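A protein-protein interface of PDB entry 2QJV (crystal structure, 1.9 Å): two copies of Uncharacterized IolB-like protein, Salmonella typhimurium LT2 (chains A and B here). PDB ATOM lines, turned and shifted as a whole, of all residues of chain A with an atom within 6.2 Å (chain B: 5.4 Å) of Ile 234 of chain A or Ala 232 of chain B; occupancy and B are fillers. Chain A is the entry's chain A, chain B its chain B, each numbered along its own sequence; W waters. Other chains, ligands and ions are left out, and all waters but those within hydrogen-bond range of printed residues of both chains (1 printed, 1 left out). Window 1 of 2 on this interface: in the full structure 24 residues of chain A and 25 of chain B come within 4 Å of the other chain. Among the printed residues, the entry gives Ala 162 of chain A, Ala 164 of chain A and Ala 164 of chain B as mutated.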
ATOM      1  N   ALA A 162      -2.377   9.019  -0.180  1.00  0.00           N
ATOM      2  CA  ALA A 162      -3.110  10.132  -0.800  1.00  0.00           C
ATOM      3  C   ALA A 162      -4.617   9.866  -0.771  1.00  0.00           C
ATOM      4  O   ALA A 162      -5.073   8.816  -1.245  1.00  0.00           O
ATOM      5  CB  ALA A 162      -2.622  10.380  -2.234  1.00  0.00           C
ATOM      6  N   GLY A 163      -5.334  10.849  -0.212  1.00  0.00           N
ATOM      7  CA  GLY A 163      -6.783  10.792  -0.045  1.00  0.00           C
ATOM      8  C   GLY A 163      -7.181  10.672   1.423  1.00  0.00           C
ATOM      9  O   GLY A 163      -8.011  11.493   1.918  1.00  0.00           O
ATOM     10  N   ALA A 164      -6.489   9.746   2.130  1.00  0.00           N
ATOM     11  CA  ALA A 164      -6.809   9.382   3.503  1.00  0.00           C
ATOM     12  C   ALA A 164      -6.588  10.526   4.496  1.00  0.00           C
ATOM     13  O   ALA A 164      -5.780  11.460   4.291  1.00  0.00           O
ATOM     14  CB  ALA A 164      -5.986   8.144   3.948  1.00  0.00           C
ATOM     15  N   PHE A 198       1.357  18.720  -1.133  1.00  0.00           N
ATOM     16  CA  PHE A 198       0.979  19.290   0.143  1.00  0.00           C
ATOM     17  C   PHE A 198      -0.201  18.510   0.737  1.00  0.00           C
ATOM     18  O   PHE A 198      -0.804  17.673   0.074  1.00  0.00           O
ATOM     19  CB  PHE A 198       0.637  20.798   0.008  1.00  0.00           C
ATOM     20  CG  PHE A 198      -0.617  21.083  -0.771  1.00  0.00           C
ATOM     21  CD1 PHE A 198      -0.567  21.288  -2.151  1.00  0.00           C
ATOM     22  CD2 PHE A 198      -1.852  21.204  -0.131  1.00  0.00           C
ATOM     23  CE1 PHE A 198      -1.735  21.595  -2.890  1.00  0.00           C
ATOM     24  CE2 PHE A 198      -3.033  21.470  -0.874  1.00  0.00           C
ATOM     25  CZ  PHE A 198      -2.968  21.681  -2.244  1.00  0.00           C
ATOM     26  N   CYS A 199      -0.445  18.768   2.017  1.00  0.00           N
ATOM     27  CA  CYS A 199      -1.608  18.300   2.729  1.00  0.00           C
ATOM     28  C   CYS A 199      -2.181  19.530   3.431  1.00  0.00           C
ATOM     29  O   CYS A 199      -1.559  20.613   3.451  1.00  0.00           O
ATOM     30  CB  CYS A 199      -1.289  17.179   3.734  1.00  0.00           C
ATOM     31  SG  CYS A 199      -0.371  17.663   5.171  1.00  0.00           S
ATOM     32  N   LEU A 200      -3.379  19.363   3.968  1.00  0.00           N
ATOM     33  CA  LEU A 200      -4.049  20.379   4.766  1.00  0.00           C
ATOM     34  C   LEU A 200      -4.189  19.849   6.203  1.00  0.00           C
ATOM     35  O   LEU A 200      -4.830  18.797   6.456  1.00  0.00           O
ATOM     36  CB  LEU A 200      -5.405  20.735   4.165  1.00  0.00           C
ATOM     37  CG  LEU A 200      -5.358  21.253   2.704  1.00  0.00           C
ATOM     38  CD1 LEU A 200      -6.761  21.475   2.135  1.00  0.00           C
ATOM     39  CD2 LEU A 200      -4.515  22.535   2.583  1.00  0.00           C
ATOM     40  N   ALA A 232      -5.437  16.099   6.545  1.00  0.00           N
ATOM     41  CA  ALA A 232      -6.169  15.721   5.326  1.00  0.00           C
ATOM     42  C   ALA A 232      -5.198  15.722   4.138  1.00  0.00           C
ATOM     43  O   ALA A 232      -4.645  16.757   3.764  1.00  0.00           O
ATOM     44  CB  ALA A 232      -7.398  16.628   5.057  1.00  0.00           C
ATOM     45  N   THR A 233      -4.979  14.551   3.563  1.00  0.00           N
ATOM     46  CA  THR A 233      -4.114  14.416   2.401  1.00  0.00           C
ATOM     47  C   THR A 233      -4.909  14.666   1.091  1.00  0.00           C
ATOM     48  O   THR A 233      -6.132  14.594   1.045  1.00  0.00           O
ATOM     49  CB  THR A 233      -3.355  13.022   2.359  1.00  0.00           C
ATOM     50  OG1 THR A 233      -4.281  11.991   2.108  1.00  0.00           O
ATOM     51  CG2 THR A 233      -2.584  12.737   3.658  1.00  0.00           C
ATOM     52  N   ILE A 234      -4.146  14.902   0.026  1.00  0.00           N
ATOM     53  CA  ILE A 234      -4.583  15.313  -1.291  1.00  0.00           C
ATOM     54  C   ILE A 234      -4.265  14.241  -2.332  1.00  0.00           C
ATOM     55  O   ILE A 234      -3.143  13.723  -2.357  1.00  0.00           O
ATOM     56  CB  ILE A 234      -3.807  16.665  -1.632  1.00  0.00           C
ATOM     57  CG1 ILE A 234      -4.226  17.780  -0.643  1.00  0.00           C
ATOM     58  CG2 ILE A 234      -3.973  17.116  -3.043  1.00  0.00           C
ATOM     59  CD1 ILE A 234      -5.675  18.129  -0.648  1.00  0.00           C
ATOM     60  N   ALA A 235      -5.251  13.897  -3.156  1.00  0.00           N
ATOM     61  CA  ALA A 235      -5.095  12.930  -4.253  1.00  0.00           C
ATOM     62  C   ALA A 235      -3.788  13.173  -5.039  1.00  0.00           C
ATOM     63  O   ALA A 235      -3.494  14.301  -5.459  1.00  0.00           O
ATOM     64  CB  ALA A 235      -6.296  12.948  -5.193  1.00  0.00           C
ATOM     65  N   GLY A 236      -3.021  12.102  -5.248  1.00  0.00           N
ATOM     66  CA  GLY A 236      -1.745  12.178  -5.958  1.00  0.00           C
ATOM     67  C   GLY A 236      -0.517  12.331  -5.093  1.00  0.00           C
ATOM     68  O   GLY A 236       0.587  11.999  -5.526  1.00  0.00           O
ATOM     69  N   TYR A 237      -0.694  12.794  -3.855  1.00  0.00           N
ATOM     70  CA  TYR A 237       0.425  13.022  -2.936  1.00  0.00           C
ATOM     71  C   TYR A 237       0.355  12.245  -1.634  1.00  0.00           C
ATOM     72  O   TYR A 237      -0.391  12.587  -0.707  1.00  0.00           O
ATOM     73  CB  TYR A 237       0.574  14.512  -2.636  1.00  0.00           C
ATOM     74  CG  TYR A 237       0.880  15.297  -3.883  1.00  0.00           C
ATOM     75  CD1 TYR A 237       2.125  15.177  -4.509  1.00  0.00           C
ATOM     76  CD2 TYR A 237      -0.054  16.172  -4.438  1.00  0.00           C
ATOM     77  CE1 TYR A 237       2.419  15.891  -5.644  1.00  0.00           C
ATOM     78  CE2 TYR A 237       0.244  16.885  -5.626  1.00  0.00           C
ATOM     79  CZ  TYR A 237       1.467  16.727  -6.203  1.00  0.00           C
ATOM     80  OH  TYR A 237       1.763  17.447  -7.346  1.00  0.00           O
ATOM     81  N   ASP A 238       1.148  11.182  -1.602  1.00  0.00           N
ATOM     82  CA  ASP A 238       1.328  10.384  -0.390  1.00  0.00           C
ATOM     83  C   ASP A 238       2.064  11.244   0.673  1.00  0.00           C
ATOM     84  O   ASP A 238       2.906  12.110   0.363  1.00  0.00           O
ATOM     85  CB  ASP A 238       2.086   9.077  -0.650  1.00  0.00           C
ATOM     86  CG  ASP A 238       1.302   8.060  -1.435  1.00  0.00           C
ATOM     87  OD1 ASP A 238       0.051   8.030  -1.420  1.00  0.00           O
ATOM     88  OD2 ASP A 238       1.986   7.273  -2.085  1.00  0.00           O
ATOM     89  N   ALA B 164     -11.734  11.661  -0.925  1.00  0.00           N
ATOM     90  CA  ALA B 164     -11.398  12.171  -2.245  1.00  0.00           C
ATOM     91  C   ALA B 164     -11.187  13.662  -2.223  1.00  0.00           C
ATOM     92  O   ALA B 164     -11.764  14.385  -1.390  1.00  0.00           O
ATOM     93  CB  ALA B 164     -12.515  11.788  -3.274  1.00  0.00           C
ATOM     94  N   THR B 165     -10.400  14.130  -3.202  1.00  0.00           N
ATOM     95  CA  THR B 165     -10.149  15.528  -3.412  1.00  0.00           C
ATOM     96  C   THR B 165     -10.908  15.978  -4.687  1.00  0.00           C
ATOM     97  O   THR B 165     -10.871  15.278  -5.692  1.00  0.00           O
ATOM     98  CB  THR B 165      -8.634  15.830  -3.601  1.00  0.00           C
ATOM     99  OG1 THR B 165      -7.831  15.064  -2.673  1.00  0.00           O
ATOM    100  CG2 THR B 165      -8.369  17.348  -3.511  1.00  0.00           C
ATOM    101  N   SER B 166     -11.585  17.116  -4.641  1.00  0.00           N
ATOM    102  CA  SER B 166     -12.258  17.652  -5.837  1.00  0.00           C
ATOM    103  C   SER B 166     -11.848  19.094  -6.057  1.00  0.00           C
ATOM    104  O   SER B 166     -11.104  19.675  -5.257  1.00  0.00           O
ATOM    105  CB  SER B 166     -13.789  17.462  -5.783  1.00  0.00           C
ATOM    106  OG  SER B 166     -14.363  18.101  -4.692  1.00  0.00           O
ATOM    107  N   TRP B 168      -9.937  19.671  -8.242  1.00  0.00           N
ATOM    108  CA  TRP B 168      -8.545  19.240  -8.167  1.00  0.00           C
ATOM    109  C   TRP B 168      -8.318  18.251  -9.323  1.00  0.00           C
ATOM    110  O   TRP B 168      -9.187  17.411  -9.584  1.00  0.00           O
ATOM    111  CB  TRP B 168      -8.287  18.598  -6.794  1.00  0.00           C
ATOM    112  CG  TRP B 168      -6.945  17.990  -6.613  1.00  0.00           C
ATOM    113  CD1 TRP B 168      -6.631  16.689  -6.746  1.00  0.00           C
ATOM    114  CD2 TRP B 168      -5.720  18.677  -6.311  1.00  0.00           C
ATOM    115  NE1 TRP B 168      -5.285  16.499  -6.540  1.00  0.00           N
ATOM    116  CE2 TRP B 168      -4.703  17.709  -6.278  1.00  0.00           C
ATOM    117  CE3 TRP B 168      -5.385  20.020  -6.061  1.00  0.00           C
ATOM    118  CZ2 TRP B 168      -3.365  18.039  -6.018  1.00  0.00           C
ATOM    119  CZ3 TRP B 168      -4.064  20.339  -5.792  1.00  0.00           C
ATOM    120  CH2 TRP B 168      -3.078  19.354  -5.760  1.00  0.00           C
ATOM    121  N   CYS B 199     -15.062  19.749   5.622  1.00  0.00           N
ATOM    122  CA  CYS B 199     -14.019  19.546   4.656  1.00  0.00           C
ATOM    123  C   CYS B 199     -13.042  20.705   4.854  1.00  0.00           C
ATOM    124  O   CYS B 199     -13.328  21.662   5.572  1.00  0.00           O
ATOM    125  CB  CYS B 199     -14.524  19.486   3.210  1.00  0.00           C
ATOM    126  SG  CYS B 199     -15.135  21.034   2.547  1.00  0.00           S
ATOM    127  N   LEU B 200     -11.896  20.612   4.190  1.00  0.00           N
ATOM    128  CA  LEU B 200     -10.903  21.664   4.201  1.00  0.00           C
ATOM    129  C   LEU B 200     -10.758  22.198   2.761  1.00  0.00           C
ATOM    130  O   LEU B 200     -10.413  21.447   1.871  1.00  0.00           O
ATOM    131  CB  LEU B 200      -9.582  21.165   4.769  1.00  0.00           C
ATOM    132  CG  LEU B 200      -9.651  20.657   6.217  1.00  0.00           C
ATOM    133  CD1 LEU B 200      -8.317  20.089   6.646  1.00  0.00           C
ATOM    134  CD2 LEU B 200     -10.100  21.762   7.189  1.00  0.00           C
ATOM    135  N   GLN B 201     -11.076  23.469   2.553  1.00  0.00           N
ATOM    136  CA  GLN B 201     -10.971  24.104   1.227  1.00  0.00           C
ATOM    137  C   GLN B 201      -9.869  25.161   1.293  1.00  0.00           C
ATOM    138  O   GLN B 201      -9.784  25.947   2.239  1.00  0.00           O
ATOM    139  CB  GLN B 201     -12.323  24.672   0.731  1.00  0.00           C
ATOM    140  CG  GLN B 201     -12.188  25.273  -0.676  1.00  0.00           C
ATOM    141  CD  GLN B 201     -13.502  25.450  -1.397  1.00  0.00           C
ATOM    142  OE1 GLN B 201     -14.545  25.462  -0.781  1.00  0.00           O
ATOM    143  NE2 GLN B 201     -13.436  25.609  -2.728  1.00  0.00           N
ATOM    144  N   PRO B 230      -8.970  24.021  -4.443  1.00  0.00           N
ATOM    145  CA  PRO B 230      -9.324  22.591  -4.186  1.00  0.00           C
ATOM    146  C   PRO B 230     -10.039  22.325  -2.849  1.00  0.00           C
ATOM    147  O   PRO B 230      -9.856  23.059  -1.861  1.00  0.00           O
ATOM    148  CB  PRO B 230      -7.978  21.885  -4.148  1.00  0.00           C
ATOM    149  CG  PRO B 230      -6.978  22.956  -3.740  1.00  0.00           C
ATOM    150  CD  PRO B 230      -7.516  24.232  -4.403  1.00  0.00           C
ATOM    151  N   VAL B 231     -10.748  21.210  -2.826  1.00  0.00           N
ATOM    152  CA  VAL B 231     -11.546  20.748  -1.683  1.00  0.00           C
ATOM    153  C   VAL B 231     -11.041  19.370  -1.229  1.00  0.00           C
ATOM    154  O   VAL B 231     -11.073  18.419  -1.993  1.00  0.00           O
ATOM    155  CB  VAL B 231     -13.072  20.674  -2.020  1.00  0.00           C
ATOM    156  CG1 VAL B 231     -13.853  19.975  -0.889  1.00  0.00           C
ATOM    157  CG2 VAL B 231     -13.651  22.077  -2.374  1.00  0.00           C
ATOM    158  N   ALA B 232     -10.544  19.299   0.008  1.00  0.00           N
ATOM    159  CA  ALA B 232     -10.071  18.056   0.613  1.00  0.00           C
ATOM    160  C   ALA B 232     -11.140  17.575   1.580  1.00  0.00           C
ATOM    161  O   ALA B 232     -11.428  18.243   2.560  1.00  0.00           O
ATOM    162  CB  ALA B 232      -8.710  18.248   1.337  1.00  0.00           C
ATOM    163  N   THR B 233     -11.771  16.433   1.283  1.00  0.00           N
ATOM    164  CA  THR B 233     -12.790  15.840   2.165  1.00  0.00           C
ATOM    165  C   THR B 233     -12.094  14.990   3.237  1.00  0.00           C
ATOM    166  O   THR B 233     -10.901  14.654   3.140  1.00  0.00           O
ATOM    167  CB  THR B 233     -13.817  14.998   1.392  1.00  0.00           C
ATOM    168  OG1 THR B 233     -13.129  13.918   0.779  1.00  0.00           O
ATOM    169  CG2 THR B 233     -14.521  15.855   0.350  1.00  0.00           C
ATOM    170  N   ILE B 234     -12.868  14.700   4.288  1.00  0.00           N
ATOM    171  CA  ILE B 234     -12.433  14.060   5.519  1.00  0.00           C
ATOM    172  C   ILE B 234     -13.077  12.687   5.656  1.00  0.00           C
ATOM    173  O   ILE B 234     -14.275  12.584   5.439  1.00  0.00           O
ATOM    174  CB  ILE B 234     -12.838  14.984   6.739  1.00  0.00           C
ATOM    175  CG1 ILE B 234     -12.129  16.364   6.688  1.00  0.00           C
ATOM    176  CG2 ILE B 234     -12.547  14.337   8.081  1.00  0.00           C
ATOM    177  CD1 ILE B 234     -10.641  16.275   6.885  1.00  0.00           C
HETATM  178  O   HOH W   1      -8.525  15.103  -0.164  1.00  0.00           O
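Among the printed residues, merely in contact across the chains: Ile 234 of chain A with Trp 168 of chain B, Ile 234 of chain A with Thr 165 of chain B, Ile 234 of chain A with Ala 232 of chain B, Leu 200 of chain A with Leu 200 of chain B, Ala 232 of chain A with Ile 234 of chain B, Tyr 237 of chain A with Trp 168 of chain B, Leu 200 of chain A with Ala 232 of chain B, Phe 198 of chain A with Trp 168 of chain B and Ala 232 of chain A with Leu 200 of chain B.
Printed residues of chain A that touch a printed residue of chain B: Phe 198, Leu 200, Ala 232, Ile 234, Ala 235 and Tyr 237. Hydrophobic or aromatic side chains of chain B that line the printed part of chain A: Trp 168, Leu 200, Ala 232 and Ile 234. Among the printed residues, no Asp or Glu carboxylate lies within 4 Å of a Lys or Arg side-chain nitrogen of the other chain.
Water W1 bridges the side-chain hydroxyl of Thr 165 of chain B (2.6 Å) and the backbone carbonyl oxygen of Thr 233 of chain A (2.7 Å).
Printed residues of chain B within 4 Å of Ile 234 of chain A: Thr 165 (3.5 Å), Trp 168 (3.2 Å) and Ala 232 (3.6 Å). Of the printed residues of chain A, Ala 232 of chain B touches Leu 200 and Ile 234. Printed residues of chain A within 4 Å of Ile 234 of chain B: Ala 232. Of the printed residues of chain A, Trp 168 of chain B touches Phe 198, Ile 234, Ala 235 and Tyr 237. Asp 238 of chain A touches none of the printed residues of chain B. The nearest residue of chain A that does not touch Ala 232 of chain B is Ala 232 of chain A (4.3 Å). The nearest printed residue of chain A that does not touch Ile 234 of chain B is Gly 163 of chain A (6.3 Å).
The backbone carbonyl oxygen of Ala 235 of chain A lies within hydrogen-bond range of the indole nitrogen of Trp 168 of chain B, at 3.0 Å. The side-chain hydroxyl (OG1) of Thr 165 of chain B lies within hydrogen-bond range of the backbone NH (N) of Ala 235 of chain A (2.9 Å).
The backbone carbonyl oxygen (O) of Leu 200 of chain B lies within hydrogen-bond range of the backbone NH (N) of Ala 232 of chain B (2.8 Å). The backbone NH of Ala 232 of chain A lies within hydrogen-bond range of the backbone carbonyl oxygen of Leu 200 of chain A (2.8 Å).
Leu 200 of chain B touches its own counterpart, Leu 200 of chain A. Leu 200 of chain A touches Ala 232 of chain B, and with the chains exchanged Ala 232 of chain A touches Leu 200 of chain B. Ala 232 of chain A touches Ile 234 of chain B, and with the chains exchanged Ile 234 of chain A touches Ala 232 of chain B. Positions printed for both chains: 164, 199, 200, 232, 233 and 234.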
